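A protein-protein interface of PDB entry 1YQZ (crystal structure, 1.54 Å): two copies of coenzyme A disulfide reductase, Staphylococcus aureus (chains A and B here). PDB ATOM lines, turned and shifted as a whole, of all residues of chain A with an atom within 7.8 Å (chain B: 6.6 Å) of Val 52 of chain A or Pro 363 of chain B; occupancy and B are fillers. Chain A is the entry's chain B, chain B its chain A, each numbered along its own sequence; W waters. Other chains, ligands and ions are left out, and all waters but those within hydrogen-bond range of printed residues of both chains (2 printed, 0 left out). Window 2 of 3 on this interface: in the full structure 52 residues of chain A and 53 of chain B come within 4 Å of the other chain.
No position is printed for both chains.
Of the 6 pairs that touch across the chains among the printed residues, none has its exchanged pair printed and touching as well.
Among the printed residues, pairs that only touch across the chains: Tyr 58 of chain A with Tyr 361 of chain B, Val 52 of chain A with Pro 363 of chain B, Tyr 47 of chain A with Tyr 362 of chain B, Val 53 of chain A with Tyr 361 of chain B and Tyr 58 of chain A with Asn 360 of chain B.
Of the 16 printed residues of chain A, 5 touch a printed residue of chain B.
Along chain A the printed residues that touch a printed residue of chain B span positions 44 to 58.
Hydrophobic or aromatic side chains of chain B within 4 Å of the printed part of chain A: Tyr 361, Tyr 362 and Pro 363.
Among the printed residues, 6 pairs touch across the chains.
A ring nitrogen (NE2) of His 358 of chain B sits at hydrogen-bond distance from the backbone carbonyl oxygen (O) of Tyr 362 of chain B.
O of Pro 363 of chain B lies within hydrogen-bond range of NE2 of His 358 of chain B.
ND2 of Asn 365 of chain B lies within hydrogen-bond range of OD1 of Asn 360 of chain B (3.3 Å).
The backbone carbonyl oxygen (O) of Tyr 47 of chain A lies within hydrogen-bond range of the backbone NH (N) of Val 52 of chain A.
The backbone NH (N) of Val 53 of chain A is in hydrogen-bond range of the backbone carbonyl oxygen (O) of Tyr 47 of chain A, at 3.0 Å.
Water W2 bridges O of Tyr 361 of chain B (2.7 Å) and O of Val 52 of chain A (3.0 Å).
Water W1 bridges OH of Tyr 362 of chain B and OE2 of Glu 165 of chain A.
OH of Tyr 361 of chain B lies within hydrogen-bond range of N of Ala 44 of chain A, 3.4 Å away.
Of chain B, only Pro 363 comes within 4 Å of Val 52 of chain A.
Pro 363 of chain B touches just one residue of chain A: Val 52.
Of the printed residues of chain A, Asn 360 of chain B touches Tyr 58.
Of the printed residues of chain B, Tyr 58 of chain A touches Asn 360 and Tyr 361.
Asn 166 of chain A touches none of the printed residues of chain B.
Asp 55 of chain A touches none of the printed residues of chain B.
The nearest residue of chain B that does not touch Val 52 of chain A is Tyr 361 of chain B (4.7 Å).
The nearest residue of chain A that does not touch Pro 363 of chain B is Val 53 of chain A (5.6 Å).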
ATOM      1  N   ALA A  44       5.205   3.615  -3.000  1.00  0.00           N
ATOM      2  CA  ALA A  44       5.706   2.275  -3.299  1.00  0.00           C
ATOM      3  C   ALA A  44       6.936   2.321  -4.187  1.00  0.00           C
ATOM      4  O   ALA A  44       7.690   1.341  -4.252  1.00  0.00           O
ATOM      5  CB  ALA A  44       4.622   1.458  -4.013  1.00  0.00           C
ATOM      6  N   PRO A  46      10.099   3.486  -4.164  1.00  0.00           N
ATOM      7  CA  PRO A  46      11.447   3.011  -3.789  1.00  0.00           C
ATOM      8  C   PRO A  46      11.473   1.484  -3.699  1.00  0.00           C
ATOM      9  O   PRO A  46      12.482   0.855  -4.001  1.00  0.00           O
ATOM     10  CB  PRO A  46      11.678   3.641  -2.407  1.00  0.00           C
ATOM     11  CG  PRO A  46      10.850   4.920  -2.481  1.00  0.00           C
ATOM     12  CD  PRO A  46       9.590   4.476  -3.188  1.00  0.00           C
ATOM     13  N   TYR A  47      10.359   0.895  -3.264  1.00  0.00           N
ATOM     14  CA  TYR A  47      10.260  -0.551  -3.104  1.00  0.00           C
ATOM     15  C   TYR A  47      10.156  -1.281  -4.436  1.00  0.00           C
ATOM     16  O   TYR A  47      10.535  -2.456  -4.532  1.00  0.00           O
ATOM     17  CB  TYR A  47       9.088  -0.889  -2.150  1.00  0.00           C
ATOM     18  CG  TYR A  47       9.237  -0.201  -0.810  1.00  0.00           C
ATOM     19  CD1 TYR A  47       8.553   0.986  -0.528  1.00  0.00           C
ATOM     20  CD2 TYR A  47      10.128  -0.684   0.155  1.00  0.00           C
ATOM     21  CE1 TYR A  47       8.762   1.672   0.676  1.00  0.00           C
ATOM     22  CE2 TYR A  47      10.341   0.000   1.351  1.00  0.00           C
ATOM     23  CZ  TYR A  47       9.657   1.175   1.611  1.00  0.00           C
ATOM     24  OH  TYR A  47       9.870   1.848   2.800  1.00  0.00           O
ATOM     25  N   VAL A  48       9.622  -0.604  -5.456  1.00  0.00           N
ATOM     26  CA  VAL A  48       9.581  -1.181  -6.791  1.00  0.00           C
ATOM     27  C   VAL A  48      11.049  -1.240  -7.269  1.00  0.00           C
ATOM     28  O   VAL A  48      11.496  -2.245  -7.804  1.00  0.00           O
ATOM     29  CB  VAL A  48       8.758  -0.311  -7.757  1.00  0.00           C
ATOM     30  CG1 VAL A  48       8.824  -0.888  -9.203  1.00  0.00           C
ATOM     31  CG2 VAL A  48       7.300  -0.266  -7.278  1.00  0.00           C
ATOM     32  N   ILE A  49      11.795  -0.157  -7.080  1.00  0.00           N
ATOM     33  CA  ILE A  49      13.206  -0.137  -7.469  1.00  0.00           C
ATOM     34  C   ILE A  49      13.990  -1.245  -6.740  1.00  0.00           C
ATOM     35  O   ILE A  49      14.873  -1.882  -7.326  1.00  0.00           O
ATOM     36  CB  ILE A  49      13.830   1.240  -7.155  1.00  0.00           C
ATOM     37  CG1 ILE A  49      13.243   2.287  -8.109  1.00  0.00           C
ATOM     38  CG2 ILE A  49      15.376   1.155  -7.228  1.00  0.00           C
ATOM     39  CD1 ILE A  49      13.579   3.728  -7.716  1.00  0.00           C
ATOM     40  N   GLY A  50      13.658  -1.498  -5.477  1.00  0.00           N
ATOM     41  CA  GLY A  50      14.359  -2.540  -4.733  1.00  0.00           C
ATOM     42  C   GLY A  50      13.917  -3.973  -5.037  1.00  0.00           C
ATOM     43  O   GLY A  50      14.453  -4.921  -4.449  1.00  0.00           O
ATOM     44  N   GLU A  51      12.939  -4.127  -5.933  1.00  0.00           N
ATOM     45  CA  GLU A  51      12.372  -5.431  -6.317  1.00  0.00           C
ATOM     46  C   GLU A  51      11.652  -6.091  -5.144  1.00  0.00           C
ATOM     47  O   GLU A  51      11.458  -7.308  -5.091  1.00  0.00           O
ATOM     48  CB  GLU A  51      13.447  -6.346  -6.936  1.00  0.00           C
ATOM     49  CG  GLU A  51      13.856  -5.846  -8.326  1.00  0.00           C
ATOM     50  CD  GLU A  51      14.971  -6.636  -8.987  1.00  0.00           C
ATOM     51  OE1 GLU A  51      15.077  -6.526 -10.218  1.00  0.00           O
ATOM     52  OE2 GLU A  51      15.741  -7.339  -8.295  1.00  0.00           O
ATOM     53  N   VAL A  52      11.251  -5.254  -4.194  1.00  0.00           N
ATOM     54  CA  VAL A  52      10.469  -5.709  -3.040  1.00  0.00           C
ATOM     55  C   VAL A  52       9.015  -5.764  -3.526  1.00  0.00           C
ATOM     56  O   VAL A  52       8.252  -6.656  -3.145  1.00  0.00           O
ATOM     57  CB  VAL A  52      10.614  -4.731  -1.850  1.00  0.00           C
ATOM     58  CG1 VAL A  52       9.600  -5.062  -0.765  1.00  0.00           C
ATOM     59  CG2 VAL A  52      12.020  -4.822  -1.282  1.00  0.00           C
ATOM     60  N   VAL A  53       8.634  -4.796  -4.364  1.00  0.00           N
ATOM     61  CA  VAL A  53       7.292  -4.755  -4.953  1.00  0.00           C
ATOM     62  C   VAL A  53       7.462  -5.073  -6.439  1.00  0.00           C
ATOM     63  O   VAL A  53       7.884  -4.218  -7.209  1.00  0.00           O
ATOM     64  CB  VAL A  53       6.662  -3.349  -4.821  1.00  0.00           C
ATOM     65  CG1 VAL A  53       5.284  -3.335  -5.489  1.00  0.00           C
ATOM     66  CG2 VAL A  53       6.551  -2.970  -3.354  1.00  0.00           C
ATOM     67  N   GLU A  54       7.127  -6.292  -6.850  1.00  0.00           N
ATOM     68  CA  GLU A  54       7.300  -6.656  -8.255  1.00  0.00           C
ATOM     69  C   GLU A  54       6.025  -6.793  -9.092  1.00  0.00           C
ATOM     70  O   GLU A  54       6.099  -6.847 -10.322  1.00  0.00           O
ATOM     71  CB  GLU A  54       8.136  -7.943  -8.348  1.00  0.00           C
ATOM     72  CG  GLU A  54       9.564  -7.752  -7.841  1.00  0.00           C
ATOM     73  CD  GLU A  54      10.423  -9.000  -7.992  1.00  0.00           C
ATOM     74  OE1 GLU A  54      10.225  -9.957  -7.217  1.00  0.00           O
ATOM     75  OE2 GLU A  54      11.287  -9.021  -8.897  1.00  0.00           O
ATOM     76  N   ASP A  55       4.858  -6.837  -8.451  1.00  0.00           N
ATOM     77  CA  ASP A  55       3.608  -6.957  -9.201  1.00  0.00           C
ATOM     78  C   ASP A  55       3.204  -5.567  -9.684  1.00  0.00           C
ATOM     79  O   ASP A  55       3.002  -4.652  -8.881  1.00  0.00           O
ATOM     80  CB  ASP A  55       2.521  -7.552  -8.304  1.00  0.00           C
ATOM     81  CG  ASP A  55       1.250  -7.890  -9.053  1.00  0.00           C
ATOM     82  OD1 ASP A  55       0.583  -8.862  -8.640  1.00  0.00           O
ATOM     83  OD2 ASP A  55       0.891  -7.197 -10.026  1.00  0.00           O
ATOM     84  N   TYR A  58       0.435  -3.322  -8.121  1.00  0.00           N
ATOM     85  CA  TYR A  58       0.695  -2.558  -6.892  1.00  0.00           C
ATOM     86  C   TYR A  58       1.377  -1.220  -7.239  1.00  0.00           C
ATOM     87  O   TYR A  58       1.359  -0.293  -6.422  1.00  0.00           O
ATOM     88  CB  TYR A  58       1.617  -3.316  -5.926  1.00  0.00           C
ATOM     89  CG  TYR A  58       0.968  -4.449  -5.168  1.00  0.00           C
ATOM     90  CD1 TYR A  58       1.582  -5.696  -5.100  1.00  0.00           C
ATOM     91  CD2 TYR A  58      -0.230  -4.259  -4.474  1.00  0.00           C
ATOM     92  CE1 TYR A  58       1.024  -6.733  -4.361  1.00  0.00           C
ATOM     93  CE2 TYR A  58      -0.797  -5.292  -3.725  1.00  0.00           C
ATOM     94  CZ  TYR A  58      -0.160  -6.522  -3.678  1.00  0.00           C
ATOM     95  OH  TYR A  58      -0.689  -7.548  -2.939  1.00  0.00           O
ATOM     96  N   GLU A 165      18.262   2.147   0.736  1.00  0.00           N
ATOM     97  CA  GLU A 165      18.011   0.828   1.308  1.00  0.00           C
ATOM     98  C   GLU A 165      17.583  -0.171   0.238  1.00  0.00           C
ATOM     99  O   GLU A 165      18.053  -1.321   0.210  1.00  0.00           O
ATOM    100  CB  GLU A 165      16.928   0.881   2.412  1.00  0.00           C
ATOM    101  CG  GLU A 165      16.631  -0.523   3.002  1.00  0.00           C
ATOM    102  CD  GLU A 165      15.751  -0.521   4.237  1.00  0.00           C
ATOM    103  OE1 GLU A 165      15.461   0.556   4.780  1.00  0.00           O
ATOM    104  OE2 GLU A 165      15.350  -1.624   4.672  1.00  0.00           O
ATOM    105  N   ASN A 166      16.697   0.266  -0.647  1.00  0.00           N
ATOM    106  CA  ASN A 166      16.205  -0.606  -1.688  1.00  0.00           C
ATOM    107  C   ASN A 166      17.263  -1.017  -2.705  1.00  0.00           C
ATOM    108  O   ASN A 166      17.268  -2.158  -3.161  1.00  0.00           O
ATOM    109  CB  ASN A 166      14.982   0.039  -2.339  1.00  0.00           C
ATOM    110  CG  ASN A 166      13.723  -0.242  -1.521  1.00  0.00           C
ATOM    111  OD1 ASN A 166      13.174  -1.338  -1.590  1.00  0.00           O
ATOM    112  ND2 ASN A 166      13.304   0.721  -0.699  1.00  0.00           N
ATOM    113  N   GLU A 169      19.224  -3.689  -0.959  1.00  0.00           N
ATOM    114  CA  GLU A 169      18.535  -4.970  -0.907  1.00  0.00           C
ATOM    115  C   GLU A 169      18.476  -5.654  -2.276  1.00  0.00           C
ATOM    116  O   GLU A 169      18.437  -6.883  -2.347  1.00  0.00           O
ATOM    117  CB  GLU A 169      17.132  -4.807  -0.315  1.00  0.00           C
ATOM    118  CG  GLU A 169      17.120  -4.400   1.166  1.00  0.00           C
ATOM    119  CD  GLU A 169      17.962  -5.311   2.066  1.00  0.00           C
ATOM    120  OE1 GLU A 169      18.156  -6.497   1.716  1.00  0.00           O
ATOM    121  OE2 GLU A 169      18.417  -4.842   3.140  1.00  0.00           O
ATOM    122  N   ARG A 170      18.479  -4.863  -3.353  1.00  0.00           N
ATOM    123  CA  ARG A 170      18.450  -5.396  -4.722  1.00  0.00           C
ATOM    124  C   ARG A 170      19.794  -6.055  -5.050  1.00  0.00           C
ATOM    125  O   ARG A 170      19.912  -6.822  -6.022  1.00  0.00           O
ATOM    126  CB  ARG A 170      18.144  -4.268  -5.723  1.00  0.00           C
ATOM    127  CG  ARG A 170      18.130  -4.690  -7.200  1.00  0.00           C
ATOM    128  CD  ARG A 170      17.464  -3.603  -8.054  1.00  0.00           C
ATOM    129  NE  ARG A 170      17.476  -3.941  -9.475  1.00  0.00           N
ATOM    130  CZ  ARG A 170      16.605  -3.488 -10.369  1.00  0.00           C
ATOM    131  NH1 ARG A 170      15.620  -2.663 -10.011  1.00  0.00           N
ATOM    132  NH2 ARG A 170      16.707  -3.870 -11.635  1.00  0.00           N
ATOM    133  N   HIS B 358      -0.578  -2.727   7.258  1.00  0.00           N
ATOM    134  CA  HIS B 358       0.217  -1.706   6.595  1.00  0.00           C
ATOM    135  C   HIS B 358      -0.026  -1.763   5.082  1.00  0.00           C
ATOM    136  O   HIS B 358      -0.942  -2.448   4.632  1.00  0.00           O
ATOM    137  CB  HIS B 358       1.709  -1.858   6.956  1.00  0.00           C
ATOM    138  CG  HIS B 358       2.306  -3.174   6.555  1.00  0.00           C
ATOM    139  ND1 HIS B 358       2.852  -4.053   7.469  1.00  0.00           N
ATOM    140  CD2 HIS B 358       2.497  -3.729   5.333  1.00  0.00           C
ATOM    141  CE1 HIS B 358       3.358  -5.092   6.825  1.00  0.00           C
ATOM    142  NE2 HIS B 358       3.160  -4.919   5.531  1.00  0.00           N
ATOM    143  N   ALA B 359       0.768  -1.042   4.288  1.00  0.00           N
ATOM    144  CA  ALA B 359       0.528  -1.022   2.834  1.00  0.00           C
ATOM    145  C   ALA B 359       0.422  -2.427   2.254  1.00  0.00           C
ATOM    146  O   ALA B 359       1.257  -3.276   2.530  1.00  0.00           O
ATOM    147  CB  ALA B 359       1.645  -0.236   2.124  1.00  0.00           C
ATOM    148  N   ASN B 360      -0.604  -2.654   1.434  1.00  0.00           N
ATOM    149  CA  ASN B 360      -0.833  -3.989   0.884  1.00  0.00           C
ATOM    150  C   ASN B 360       0.319  -4.564   0.074  1.00  0.00           C
ATOM    151  O   ASN B 360       0.486  -5.785   0.018  1.00  0.00           O
ATOM    152  CB  ASN B 360      -2.123  -4.013   0.060  1.00  0.00           C
ATOM    153  CG  ASN B 360      -3.350  -3.700   0.902  1.00  0.00           C
ATOM    154  OD1 ASN B 360      -3.355  -3.918   2.117  1.00  0.00           O
ATOM    155  ND2 ASN B 360      -4.396  -3.193   0.261  1.00  0.00           N
ATOM    156  N   TYR B 361       1.119  -3.690  -0.531  1.00  0.00           N
ATOM    157  CA  TYR B 361       2.259  -4.128  -1.336  1.00  0.00           C
ATOM    158  C   TYR B 361       3.522  -4.337  -0.513  1.00  0.00           C
ATOM    159  O   TYR B 361       4.535  -4.827  -1.020  1.00  0.00           O
ATOM    160  CB  TYR B 361       2.543  -3.101  -2.442  1.00  0.00           C
ATOM    161  CG  TYR B 361       2.672  -1.671  -1.944  1.00  0.00           C
ATOM    162  CD1 TYR B 361       3.826  -1.242  -1.279  1.00  0.00           C
ATOM    163  CD2 TYR B 361       1.654  -0.749  -2.165  1.00  0.00           C
ATOM    164  CE1 TYR B 361       3.956   0.079  -0.856  1.00  0.00           C
ATOM    165  CE2 TYR B 361       1.768   0.564  -1.747  1.00  0.00           C
ATOM    166  CZ  TYR B 361       2.922   0.968  -1.095  1.00  0.00           C
ATOM    167  OH  TYR B 361       3.042   2.266  -0.706  1.00  0.00           O
ATOM    168  N   TYR B 362       3.488  -3.955   0.761  1.00  0.00           N
ATOM    169  CA  TYR B 362       4.679  -4.121   1.570  1.00  0.00           C
ATOM    170  C   TYR B 362       4.659  -5.491   2.237  1.00  0.00           C
ATOM    171  O   TYR B 362       3.666  -5.879   2.871  1.00  0.00           O
ATOM    172  CB  TYR B 362       4.789  -2.991   2.598  1.00  0.00           C
ATOM    173  CG  TYR B 362       6.136  -2.937   3.252  1.00  0.00           C
ATOM    174  CD1 TYR B 362       7.232  -2.334   2.608  1.00  0.00           C
ATOM    175  CD2 TYR B 362       6.345  -3.510   4.500  1.00  0.00           C
ATOM    176  CE1 TYR B 362       8.489  -2.312   3.199  1.00  0.00           C
ATOM    177  CE2 TYR B 362       7.600  -3.491   5.100  1.00  0.00           C
ATOM    178  CZ  TYR B 362       8.667  -2.890   4.439  1.00  0.00           C
ATOM    179  OH  TYR B 362       9.907  -2.887   5.030  1.00  0.00           O
ATOM    180  N   PRO B 363       5.759  -6.245   2.101  1.00  0.00           N
ATOM    181  CA  PRO B 363       5.888  -7.592   2.662  1.00  0.00           C
ATOM    182  C   PRO B 363       5.492  -7.797   4.104  1.00  0.00           C
ATOM    183  O   PRO B 363       5.562  -6.882   4.926  1.00  0.00           O
ATOM    184  CB  PRO B 363       7.359  -7.930   2.433  1.00  0.00           C
ATOM    185  CG  PRO B 363       7.677  -7.184   1.193  1.00  0.00           C
ATOM    186  CD  PRO B 363       7.015  -5.844   1.442  1.00  0.00           C
ATOM    187  N   GLY B 364       5.079  -9.027   4.386  1.00  0.00           N
ATOM    188  CA  GLY B 364       4.689  -9.403   5.728  1.00  0.00           C
ATOM    189  C   GLY B 364       3.409  -8.773   6.219  1.00  0.00           C
ATOM    190  O   GLY B 364       3.231  -8.617   7.426  1.00  0.00           O
ATOM    191  N   ASN B 365       2.514  -8.415   5.306  1.00  0.00           N
ATOM    192  CA  ASN B 365       1.257  -7.799   5.725  1.00  0.00           C
ATOM    193  C   ASN B 365       0.310  -8.870   6.255  1.00  0.00           C
ATOM    194  O   ASN B 365       0.476 -10.069   5.984  1.00  0.00           O
ATOM    195  CB  ASN B 365       0.605  -7.061   4.555  1.00  0.00           C
ATOM    196  CG  ASN B 365      -0.332  -5.962   5.001  1.00  0.00           C
ATOM    197  OD1 ASN B 365      -0.268  -5.507   6.139  1.00  0.00           O
ATOM    198  ND2 ASN B 365      -1.199  -5.517   4.098  1.00  0.00           N
ATOM    199  N   GLU B 390      -0.442  -8.083  13.436  1.00  0.00           N
ATOM    200  CA  GLU B 390       0.301  -6.831  13.496  1.00  0.00           C
ATOM    201  C   GLU B 390      -0.594  -5.605  13.664  1.00  0.00           C
ATOM    202  O   GLU B 390      -1.664  -5.539  13.080  1.00  0.00           O
ATOM    203  CB  GLU B 390       1.113  -6.646  12.182  1.00  0.00           C
ATOM    204  CG  GLU B 390       1.806  -5.269  12.000  1.00  0.00           C
ATOM    205  CD  GLU B 390       2.585  -5.136  10.678  1.00  0.00           C
ATOM    206  OE1 GLU B 390       2.739  -3.994  10.184  1.00  0.00           O
ATOM    207  OE2 GLU B 390       3.055  -6.166  10.143  1.00  0.00           O
HETATM  208  O   HOH W   1      12.298  -1.778   3.290  1.00  0.00           O
HETATM  209  O   HOH W   2       5.222  -6.698  -2.900  1.00  0.00           O
